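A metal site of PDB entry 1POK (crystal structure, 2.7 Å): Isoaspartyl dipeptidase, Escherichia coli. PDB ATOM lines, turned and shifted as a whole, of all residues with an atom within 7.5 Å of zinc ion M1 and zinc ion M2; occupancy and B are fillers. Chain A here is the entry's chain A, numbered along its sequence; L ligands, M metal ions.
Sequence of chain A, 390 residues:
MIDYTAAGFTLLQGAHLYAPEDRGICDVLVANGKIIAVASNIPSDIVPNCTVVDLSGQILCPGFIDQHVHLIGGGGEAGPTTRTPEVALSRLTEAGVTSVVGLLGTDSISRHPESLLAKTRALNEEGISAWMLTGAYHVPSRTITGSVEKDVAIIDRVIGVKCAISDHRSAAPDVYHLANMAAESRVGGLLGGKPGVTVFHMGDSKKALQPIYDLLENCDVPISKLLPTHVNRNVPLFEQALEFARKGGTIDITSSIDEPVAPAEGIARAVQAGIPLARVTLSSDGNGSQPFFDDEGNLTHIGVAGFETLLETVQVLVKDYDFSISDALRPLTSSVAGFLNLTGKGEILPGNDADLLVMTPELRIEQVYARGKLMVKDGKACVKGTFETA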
ATOM      1  N   HIS A  68     -20.741  14.783  19.811  1.00  0.00           N
ATOM      2  CA  HIS A  68     -20.341  16.171  19.566  1.00  0.00           C
ATOM      3  C   HIS A  68     -21.471  16.890  18.827  1.00  0.00           C
ATOM      4  O   HIS A  68     -21.417  17.053  17.607  1.00  0.00           O
ATOM      5  CB  HIS A  68     -19.048  16.179  18.735  1.00  0.00           C
ATOM      6  CG  HIS A  68     -18.291  17.472  18.820  1.00  0.00           C
ATOM      7  ND1 HIS A  68     -16.942  17.557  18.524  1.00  0.00           N
ATOM      8  CD2 HIS A  68     -18.676  18.710  19.167  1.00  0.00           C
ATOM      9  CE1 HIS A  68     -16.544  18.801  18.705  1.00  0.00           C
ATOM     10  NE2 HIS A  68     -17.570  19.528  19.091  1.00  0.00           N
ATOM     11  N   VAL A  69     -22.484  17.324  19.572  1.00  0.00           N
ATOM     12  CA  VAL A  69     -23.627  18.014  18.978  1.00  0.00           C
ATOM     13  C   VAL A  69     -24.057  19.263  19.776  1.00  0.00           C
ATOM     14  O   VAL A  69     -24.222  19.221  20.994  1.00  0.00           O
ATOM     15  CB  VAL A  69     -24.840  17.038  18.847  1.00  0.00           C
ATOM     16  CG1 VAL A  69     -26.056  17.772  18.313  1.00  0.00           C
ATOM     17  CG2 VAL A  69     -24.490  15.886  17.930  1.00  0.00           C
ATOM     18  N   HIS A  70     -24.217  20.382  19.073  1.00  0.00           N
ATOM     19  CA  HIS A  70     -24.622  21.636  19.693  1.00  0.00           C
ATOM     20  C   HIS A  70     -26.133  21.715  19.846  1.00  0.00           C
ATOM     21  O   HIS A  70     -26.780  22.553  19.217  1.00  0.00           O
ATOM     22  CB  HIS A  70     -24.093  22.805  18.868  1.00  0.00           C
ATOM     23  CG  HIS A  70     -22.606  22.909  18.893  1.00  0.00           C
ATOM     24  ND1 HIS A  70     -21.922  23.629  19.851  1.00  0.00           N
ATOM     25  CD2 HIS A  70     -21.661  22.296  18.145  1.00  0.00           C
ATOM     26  CE1 HIS A  70     -20.627  23.444  19.697  1.00  0.00           C
ATOM     27  NE2 HIS A  70     -20.436  22.631  18.671  1.00  0.00           N
ATOM     28  N   GLU A  77     -19.843  33.410  15.912  1.00  0.00           N
ATOM     29  CA  GLU A  77     -18.498  33.927  15.660  1.00  0.00           C
ATOM     30  C   GLU A  77     -18.440  35.090  14.675  1.00  0.00           C
ATOM     31  O   GLU A  77     -17.417  35.767  14.562  1.00  0.00           O
ATOM     32  CB  GLU A  77     -17.593  32.773  15.224  1.00  0.00           C
ATOM     33  CG  GLU A  77     -17.505  31.682  16.284  1.00  0.00           C
ATOM     34  CD  GLU A  77     -16.966  30.361  15.754  1.00  0.00           C
ATOM     35  OE1 GLU A  77     -15.855  30.360  15.183  1.00  0.00           O
ATOM     36  OE2 GLU A  77     -17.667  29.330  15.917  1.00  0.00           O
ATOM     37  N   LEU A 103     -22.558  19.618  23.793  1.00  0.00           N
ATOM     38  CA  LEU A 103     -21.527  20.476  24.339  1.00  0.00           C
ATOM     39  C   LEU A 103     -21.750  21.895  23.822  1.00  0.00           C
ATOM     40  O   LEU A 103     -22.657  22.124  23.005  1.00  0.00           O
ATOM     41  CB  LEU A 103     -20.106  19.972  23.971  1.00  0.00           C
ATOM     42  CG  LEU A 103     -19.656  19.625  22.541  1.00  0.00           C
ATOM     43  CD1 LEU A 103     -19.750  18.120  22.353  1.00  0.00           C
ATOM     44  CD2 LEU A 103     -20.470  20.363  21.501  1.00  0.00           C
ATOM     45  N   LEU A 104     -20.950  22.836  24.303  1.00  0.00           N
ATOM     46  CA  LEU A 104     -21.054  24.222  23.872  1.00  0.00           C
ATOM     47  C   LEU A 104     -19.764  24.547  23.147  1.00  0.00           C
ATOM     48  O   LEU A 104     -18.805  23.784  23.249  1.00  0.00           O
ATOM     49  CB  LEU A 104     -21.250  25.135  25.098  1.00  0.00           C
ATOM     50  CG  LEU A 104     -22.575  24.971  25.839  1.00  0.00           C
ATOM     51  CD1 LEU A 104     -22.575  25.885  27.044  1.00  0.00           C
ATOM     52  CD2 LEU A 104     -23.735  25.303  24.916  1.00  0.00           C
ATOM     53  N   GLY A 105     -19.741  25.657  22.426  1.00  0.00           N
ATOM     54  CA  GLY A 105     -18.541  25.997  21.691  1.00  0.00           C
ATOM     55  C   GLY A 105     -17.949  27.359  22.023  1.00  0.00           C
ATOM     56  O   GLY A 105     -17.855  27.748  23.192  1.00  0.00           O
ATOM     57  N   THR A 106     -17.542  28.076  20.983  1.00  0.00           N
ATOM     58  CA  THR A 106     -16.967  29.389  21.133  1.00  0.00           C
ATOM     59  C   THR A 106     -17.791  30.298  22.073  1.00  0.00           C
ATOM     60  O   THR A 106     -17.248  30.880  23.018  1.00  0.00           O
ATOM     61  CB  THR A 106     -16.841  30.086  19.756  1.00  0.00           C
ATOM     62  OG1 THR A 106     -16.326  29.173  18.787  1.00  0.00           O
ATOM     63  CG2 THR A 106     -15.905  31.279  19.853  1.00  0.00           C
ATOM     64  N   TYR A 137     -15.394  26.339  25.255  1.00  0.00           N
ATOM     65  CA  TYR A 137     -14.040  26.688  24.810  1.00  0.00           C
ATOM     66  C   TYR A 137     -13.292  27.358  25.949  1.00  0.00           C
ATOM     67  O   TYR A 137     -12.171  26.972  26.282  1.00  0.00           O
ATOM     68  CB  TYR A 137     -14.052  27.693  23.649  1.00  0.00           C
ATOM     69  CG  TYR A 137     -14.289  27.143  22.271  1.00  0.00           C
ATOM     70  CD1 TYR A 137     -13.746  27.790  21.149  1.00  0.00           C
ATOM     71  CD2 TYR A 137     -15.085  26.015  22.058  1.00  0.00           C
ATOM     72  CE1 TYR A 137     -13.989  27.326  19.851  1.00  0.00           C
ATOM     73  CE2 TYR A 137     -15.342  25.549  20.757  1.00  0.00           C
ATOM     74  CZ  TYR A 137     -14.793  26.207  19.666  1.00  0.00           C
ATOM     75  OH  TYR A 137     -15.089  25.767  18.386  1.00  0.00           O
ATOM     76  N   KCX A 162     -15.720  20.056  28.404  1.00  0.00           N
ATOM     77  CA  KCX A 162     -15.262  20.492  27.086  1.00  0.00           C
ATOM     78  CB  KCX A 162     -16.476  20.961  26.281  1.00  0.00           C
ATOM     79  CG  KCX A 162     -16.154  21.713  24.972  1.00  0.00           C
ATOM     80  CD  KCX A 162     -15.621  20.778  23.906  1.00  0.00           C
ATOM     81  CE  KCX A 162     -15.272  21.519  22.615  1.00  0.00           C
ATOM     82  NZ  KCX A 162     -16.424  21.907  21.801  1.00  0.00           N
ATOM     83  C   KCX A 162     -14.276  21.635  27.229  1.00  0.00           C
ATOM     84  O   KCX A 162     -14.217  22.302  28.253  1.00  0.00           O
ATOM     85  CX  KCX A 162     -16.411  21.995  20.466  1.00  0.00           C
ATOM     86  OQ1 KCX A 162     -15.376  21.736  19.802  1.00  0.00           O
ATOM     87  OQ2 KCX A 162     -17.440  22.351  19.822  1.00  0.00           O
ATOM     88  N   CYS A 163     -13.504  21.883  26.185  1.00  0.00           N
ATOM     89  CA  CYS A 163     -12.545  22.991  26.216  1.00  0.00           C
ATOM     90  C   CYS A 163     -11.933  23.132  24.833  1.00  0.00           C
ATOM     91  O   CYS A 163     -12.121  22.271  23.988  1.00  0.00           O
ATOM     92  CB  CYS A 163     -11.442  22.732  27.237  1.00  0.00           C
ATOM     93  SG  CYS A 163     -10.126  21.650  26.652  1.00  0.00           S
ATOM     94  N   ALA A 164     -11.211  24.227  24.621  1.00  0.00           N
ATOM     95  CA  ALA A 164     -10.551  24.441  23.349  1.00  0.00           C
ATOM     96  C   ALA A 164      -9.099  24.772  23.596  1.00  0.00           C
ATOM     97  O   ALA A 164      -8.764  25.446  24.570  1.00  0.00           O
ATOM     98  CB  ALA A 164     -11.188  25.564  22.567  1.00  0.00           C
ATOM     99  N   ASP A 167      -6.262  27.038  19.373  1.00  0.00           N
ATOM    100  CA  ASP A 167      -7.242  27.628  18.473  1.00  0.00           C
ATOM    101  C   ASP A 167      -7.253  29.136  18.703  1.00  0.00           C
ATOM    102  O   ASP A 167      -7.097  29.598  19.832  1.00  0.00           O
ATOM    103  CB  ASP A 167      -8.629  27.055  18.769  1.00  0.00           C
ATOM    104  CG  ASP A 167      -9.630  27.396  17.688  1.00  0.00           C
ATOM    105  OD1 ASP A 167      -9.760  26.606  16.719  1.00  0.00           O
ATOM    106  OD2 ASP A 167     -10.270  28.460  17.811  1.00  0.00           O
ATOM    107  N   ARG A 169      -9.595  30.985  18.928  1.00  0.00           N
ATOM    108  CA  ARG A 169     -10.806  31.361  19.651  1.00  0.00           C
ATOM    109  C   ARG A 169     -10.738  30.789  21.072  1.00  0.00           C
ATOM    110  O   ARG A 169     -11.722  30.758  21.796  1.00  0.00           O
ATOM    111  CB  ARG A 169     -12.022  30.814  18.909  1.00  0.00           C
ATOM    112  CG  ARG A 169     -12.083  31.279  17.478  1.00  0.00           C
ATOM    113  CD  ARG A 169     -13.040  30.471  16.629  1.00  0.00           C
ATOM    114  NE  ARG A 169     -12.614  29.079  16.458  1.00  0.00           N
ATOM    115  CZ  ARG A 169     -12.806  28.359  15.351  1.00  0.00           C
ATOM    116  NH1 ARG A 169     -13.447  28.889  14.309  1.00  0.00           N
ATOM    117  NH2 ARG A 169     -12.375  27.106  15.299  1.00  0.00           N
ATOM    118  N   PHE A 200     -11.117  17.966  24.046  1.00  0.00           N
ATOM    119  CA  PHE A 200     -10.415  19.127  23.539  1.00  0.00           C
ATOM    120  C   PHE A 200     -10.793  19.489  22.132  1.00  0.00           C
ATOM    121  O   PHE A 200     -10.763  18.640  21.229  1.00  0.00           O
ATOM    122  CB  PHE A 200      -8.910  18.923  23.586  1.00  0.00           C
ATOM    123  CG  PHE A 200      -8.382  18.632  24.951  1.00  0.00           C
ATOM    124  CD1 PHE A 200      -8.589  17.400  25.547  1.00  0.00           C
ATOM    125  CD2 PHE A 200      -7.672  19.612  25.637  1.00  0.00           C
ATOM    126  CE1 PHE A 200      -8.099  17.144  26.826  1.00  0.00           C
ATOM    127  CE2 PHE A 200      -7.169  19.367  26.912  1.00  0.00           C
ATOM    128  CZ  PHE A 200      -7.389  18.123  27.512  1.00  0.00           C
ATOM    129  N   HIS A 201     -11.139  20.754  21.930  1.00  0.00           N
ATOM    130  CA  HIS A 201     -11.490  21.258  20.611  1.00  0.00           C
ATOM    131  C   HIS A 201     -10.170  21.663  19.975  1.00  0.00           C
ATOM    132  O   HIS A 201      -9.569  22.671  20.369  1.00  0.00           O
ATOM    133  CB  HIS A 201     -12.404  22.478  20.702  1.00  0.00           C
ATOM    134  CG  HIS A 201     -12.516  23.235  19.412  1.00  0.00           C
ATOM    135  ND1 HIS A 201     -13.413  22.897  18.422  1.00  0.00           N
ATOM    136  CD2 HIS A 201     -11.799  24.284  18.939  1.00  0.00           C
ATOM    137  CE1 HIS A 201     -13.251  23.720  17.396  1.00  0.00           C
ATOM    138  NE2 HIS A 201     -12.279  24.572  17.686  1.00  0.00           N
ATOM    139  N   MET A 202      -9.717  20.884  19.003  1.00  0.00           N
ATOM    140  CA  MET A 202      -8.461  21.184  18.347  1.00  0.00           C
ATOM    141  C   MET A 202      -8.583  22.300  17.320  1.00  0.00           C
ATOM    142  O   MET A 202      -9.505  22.318  16.489  1.00  0.00           O
ATOM    143  CB  MET A 202      -7.904  19.911  17.696  1.00  0.00           C
ATOM    144  CG  MET A 202      -7.549  18.845  18.698  1.00  0.00           C
ATOM    145  SD  MET A 202      -6.631  19.528  20.083  1.00  0.00           S
ATOM    146  CE  MET A 202      -5.082  19.948  19.309  1.00  0.00           C
ATOM    147  N   THR A 229     -10.565  16.404  19.469  1.00  0.00           N
ATOM    148  CA  THR A 229     -11.564  16.347  18.390  1.00  0.00           C
ATOM    149  C   THR A 229     -11.166  17.184  17.193  1.00  0.00           C
ATOM    150  O   THR A 229     -10.304  18.057  17.297  1.00  0.00           O
ATOM    151  CB  THR A 229     -12.931  16.840  18.858  1.00  0.00           C
ATOM    152  OG1 THR A 229     -13.329  16.117  20.025  1.00  0.00           O
ATOM    153  CG2 THR A 229     -13.970  16.586  17.800  1.00  0.00           C
ATOM    154  N   HIS A 230     -11.792  16.915  16.050  1.00  0.00           N
ATOM    155  CA  HIS A 230     -11.517  17.640  14.808  1.00  0.00           C
ATOM    156  C   HIS A 230     -10.084  17.361  14.389  1.00  0.00           C
ATOM    157  O   HIS A 230      -9.462  18.158  13.699  1.00  0.00           O
ATOM    158  CB  HIS A 230     -11.703  19.133  15.039  1.00  0.00           C
ATOM    159  CG  HIS A 230     -13.022  19.487  15.638  1.00  0.00           C
ATOM    160  ND1 HIS A 230     -13.166  20.484  16.591  1.00  0.00           N
ATOM    161  CD2 HIS A 230     -14.263  19.000  15.410  1.00  0.00           C
ATOM    162  CE1 HIS A 230     -14.446  20.576  16.921  1.00  0.00           C
ATOM    163  NE2 HIS A 230     -15.134  19.695  16.216  1.00  0.00           N
ATOM    164  N   ARG A 233      -8.609  18.114  10.891  1.00  0.00           N
ATOM    165  CA  ARG A 233      -8.752  19.481  10.387  1.00  0.00           C
ATOM    166  C   ARG A 233      -7.514  20.017   9.678  1.00  0.00           C
ATOM    167  O   ARG A 233      -7.590  21.010   8.971  1.00  0.00           O
ATOM    168  CB  ARG A 233      -9.171  20.410  11.508  1.00  0.00           C
ATOM    169  CG  ARG A 233      -8.154  20.564  12.616  1.00  0.00           C
ATOM    170  CD  ARG A 233      -8.649  21.581  13.607  1.00  0.00           C
ATOM    171  NE  ARG A 233      -9.073  22.768  12.903  1.00  0.00           N
ATOM    172  CZ  ARG A 233     -10.122  23.497  13.260  1.00  0.00           C
ATOM    173  NH1 ARG A 233     -10.826  23.150  14.320  1.00  0.00           N
ATOM    174  NH2 ARG A 233     -10.466  24.561  12.538  1.00  0.00           N
ATOM    175  N   THR A 254     -14.257  14.163  13.035  1.00  0.00           N
ATOM    176  CA  THR A 254     -15.584  14.748  12.790  1.00  0.00           C
ATOM    177  C   THR A 254     -15.939  14.613  11.318  1.00  0.00           C
ATOM    178  O   THR A 254     -15.209  15.073  10.441  1.00  0.00           O
ATOM    179  CB  THR A 254     -15.647  16.238  13.197  1.00  0.00           C
ATOM    180  OG1 THR A 254     -14.403  16.871  12.868  1.00  0.00           O
ATOM    181  CG2 THR A 254     -15.912  16.373  14.706  1.00  0.00           C
ATOM    182  N   SER A 284     -20.187  14.256  14.698  1.00  0.00           N
ATOM    183  CA  SER A 284     -20.697  15.125  13.638  1.00  0.00           C
ATOM    184  C   SER A 284     -20.478  16.626  13.801  1.00  0.00           C
ATOM    185  O   SER A 284     -20.408  17.364  12.832  1.00  0.00           O
ATOM    186  CB  SER A 284     -22.208  14.890  13.472  1.00  0.00           C
ATOM    187  OG  SER A 284     -22.939  15.465  14.548  1.00  0.00           O
ATOM    188  N   ASP A 285     -20.376  17.083  15.043  1.00  0.00           N
ATOM    189  CA  ASP A 285     -20.222  18.518  15.287  1.00  0.00           C
ATOM    190  C   ASP A 285     -21.511  19.142  14.743  1.00  0.00           C
ATOM    191  O   ASP A 285     -21.483  20.226  14.153  1.00  0.00           O
ATOM    192  CB  ASP A 285     -19.013  19.096  14.536  1.00  0.00           C
ATOM    193  CG  ASP A 285     -18.491  20.376  15.178  1.00  0.00           C
ATOM    194  OD1 ASP A 285     -19.312  21.124  15.752  1.00  0.00           O
ATOM    195  OD2 ASP A 285     -17.275  20.624  15.104  1.00  0.00           O
ATOM    196  N   GLY A 286     -22.634  18.455  14.945  1.00  0.00           N
ATOM    197  CA  GLY A 286     -23.916  18.930  14.468  1.00  0.00           C
ATOM    198  C   GLY A 286     -24.462  20.228  15.050  1.00  0.00           C
ATOM    199  O   GLY A 286     -24.273  20.539  16.229  1.00  0.00           O
ATOM    200  N   GLY A 288     -23.602  23.256  14.698  1.00  0.00           N
ATOM    201  CA  GLY A 288     -22.705  24.360  14.975  1.00  0.00           C
ATOM    202  C   GLY A 288     -22.363  24.994  13.642  1.00  0.00           C
ATOM    203  O   GLY A 288     -23.164  24.971  12.702  1.00  0.00           O
ATOM    204  N   SER A 289     -21.164  25.563  13.564  1.00  0.00           N
ATOM    205  CA  SER A 289     -20.675  26.192  12.335  1.00  0.00           C
ATOM    206  C   SER A 289     -19.441  27.003  12.678  1.00  0.00           C
ATOM    207  O   SER A 289     -19.026  27.043  13.839  1.00  0.00           O
ATOM    208  CB  SER A 289     -21.740  27.104  11.734  1.00  0.00           C
ATOM    209  OG  SER A 289     -21.423  27.388  10.385  1.00  0.00           O
HETATM  210  N1  LIG L   1     -14.859  25.844  15.194  1.00  0.00           N
HETATM  211  C1  LIG L   1     -15.073  25.246  13.850  1.00  0.00           C
HETATM  212  C2  LIG L   1     -15.582  23.803  13.940  1.00  0.00           C
HETATM  213  O1  LIG L   1     -16.125  23.423  15.002  1.00  0.00           O
HETATM  214  C3  LIG L   1     -13.769  25.295  13.039  1.00  0.00           C
HETATM  215  C4  LIG L   1     -13.705  26.504  12.115  1.00  0.00           C
HETATM  216  O2  LIG L   1     -12.636  27.084  11.888  1.00  0.00           O
HETATM  217  N2  LIG L   1     -14.861  26.881  11.554  1.00  0.00           N
HETATM  218  O3  LIG L   1     -15.425  23.068  12.936  1.00  0.00           O
HETATM  219 ZN    ZN M   1     -18.254  21.867  17.998  1.00  0.00          ZN
HETATM  220 ZN    ZN M   2     -15.366  22.523  17.949  1.00  0.00          ZN
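OH of Tyr 137 touches zinc ion M2, at 3.3 Å. His 230 touches zinc ion M2. Within 4 Å of zinc ion M2: His 68, Tyr 137, KCX 162, His 201, His 230 and Asp 285. The nearest printed residue that does not touch zinc ion M2 is His 70 (5.1 Å).
O of His 68 lies within hydrogen-bond range of N of Gly 286, 3.2 Å away. The backbone carbonyl oxygen (O) of Leu 104 is in hydrogen-bond range of NZ of KCX 162. The backbone carbonyl oxygen (O) of Tyr 137 lies within hydrogen-bond range of the backbone NH (N) of Ala 164 (3.3 Å). A ring nitrogen (ND1) of His 201 lies close to a ring nitrogen (ND1) of His 230, at 3.0 Å. NE2 of His 201 lies within hydrogen-bond range of NH2 of Arg 169 (3.5 Å). OD1 of Asp 167 lies within hydrogen-bond range of NE2 of His 201, 3.4 Å away. The backbone NH (N) of His 70 is in hydrogen-bond range of the backbone carbonyl oxygen (O) of Gly 286. NE2 of His 230 lies within hydrogen-bond range of OD2 of Asp 285.
Zinc ion M1 is bound by OQ2 of KCX 162 (2.1 Å), a ring nitrogen (NE2) of His 70 (2.4 Å), the side-chain carboxylate of Asp 285 (2.6 Å) and a ring nitrogen (NE2) of His 68 (2.7 Å). Zinc ion M1 has four donor atoms within binding distance.
Of the 26 residues printed, 4 come within 4 Å of zinc ion M1.
Zinc ion M2 is bound by OQ1 of KCX 162 (2.0 Å) and ND1 of His 201 (2.0 Å). Zinc ion M2 has two donor atoms within binding distance. Slightly farther from zinc ion M2 lies OQ2 of KCX 162 (2.8 Å).
O1 of the ligand sits close to OD2 of Asp 285 (3.0 Å). NH1 of Arg 169 sits at hydrogen-bond distance from O2 of the ligand (3.1 Å). A nitrogen (N1) of the ligand lies within hydrogen-bond range of the side-chain hydroxyl (OH) of Tyr 137 (3.2 Å). The guanidinium group of Arg 233 sits at hydrogen-bond distance from an oxygen (O2) of the ligand (3.4 Å).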
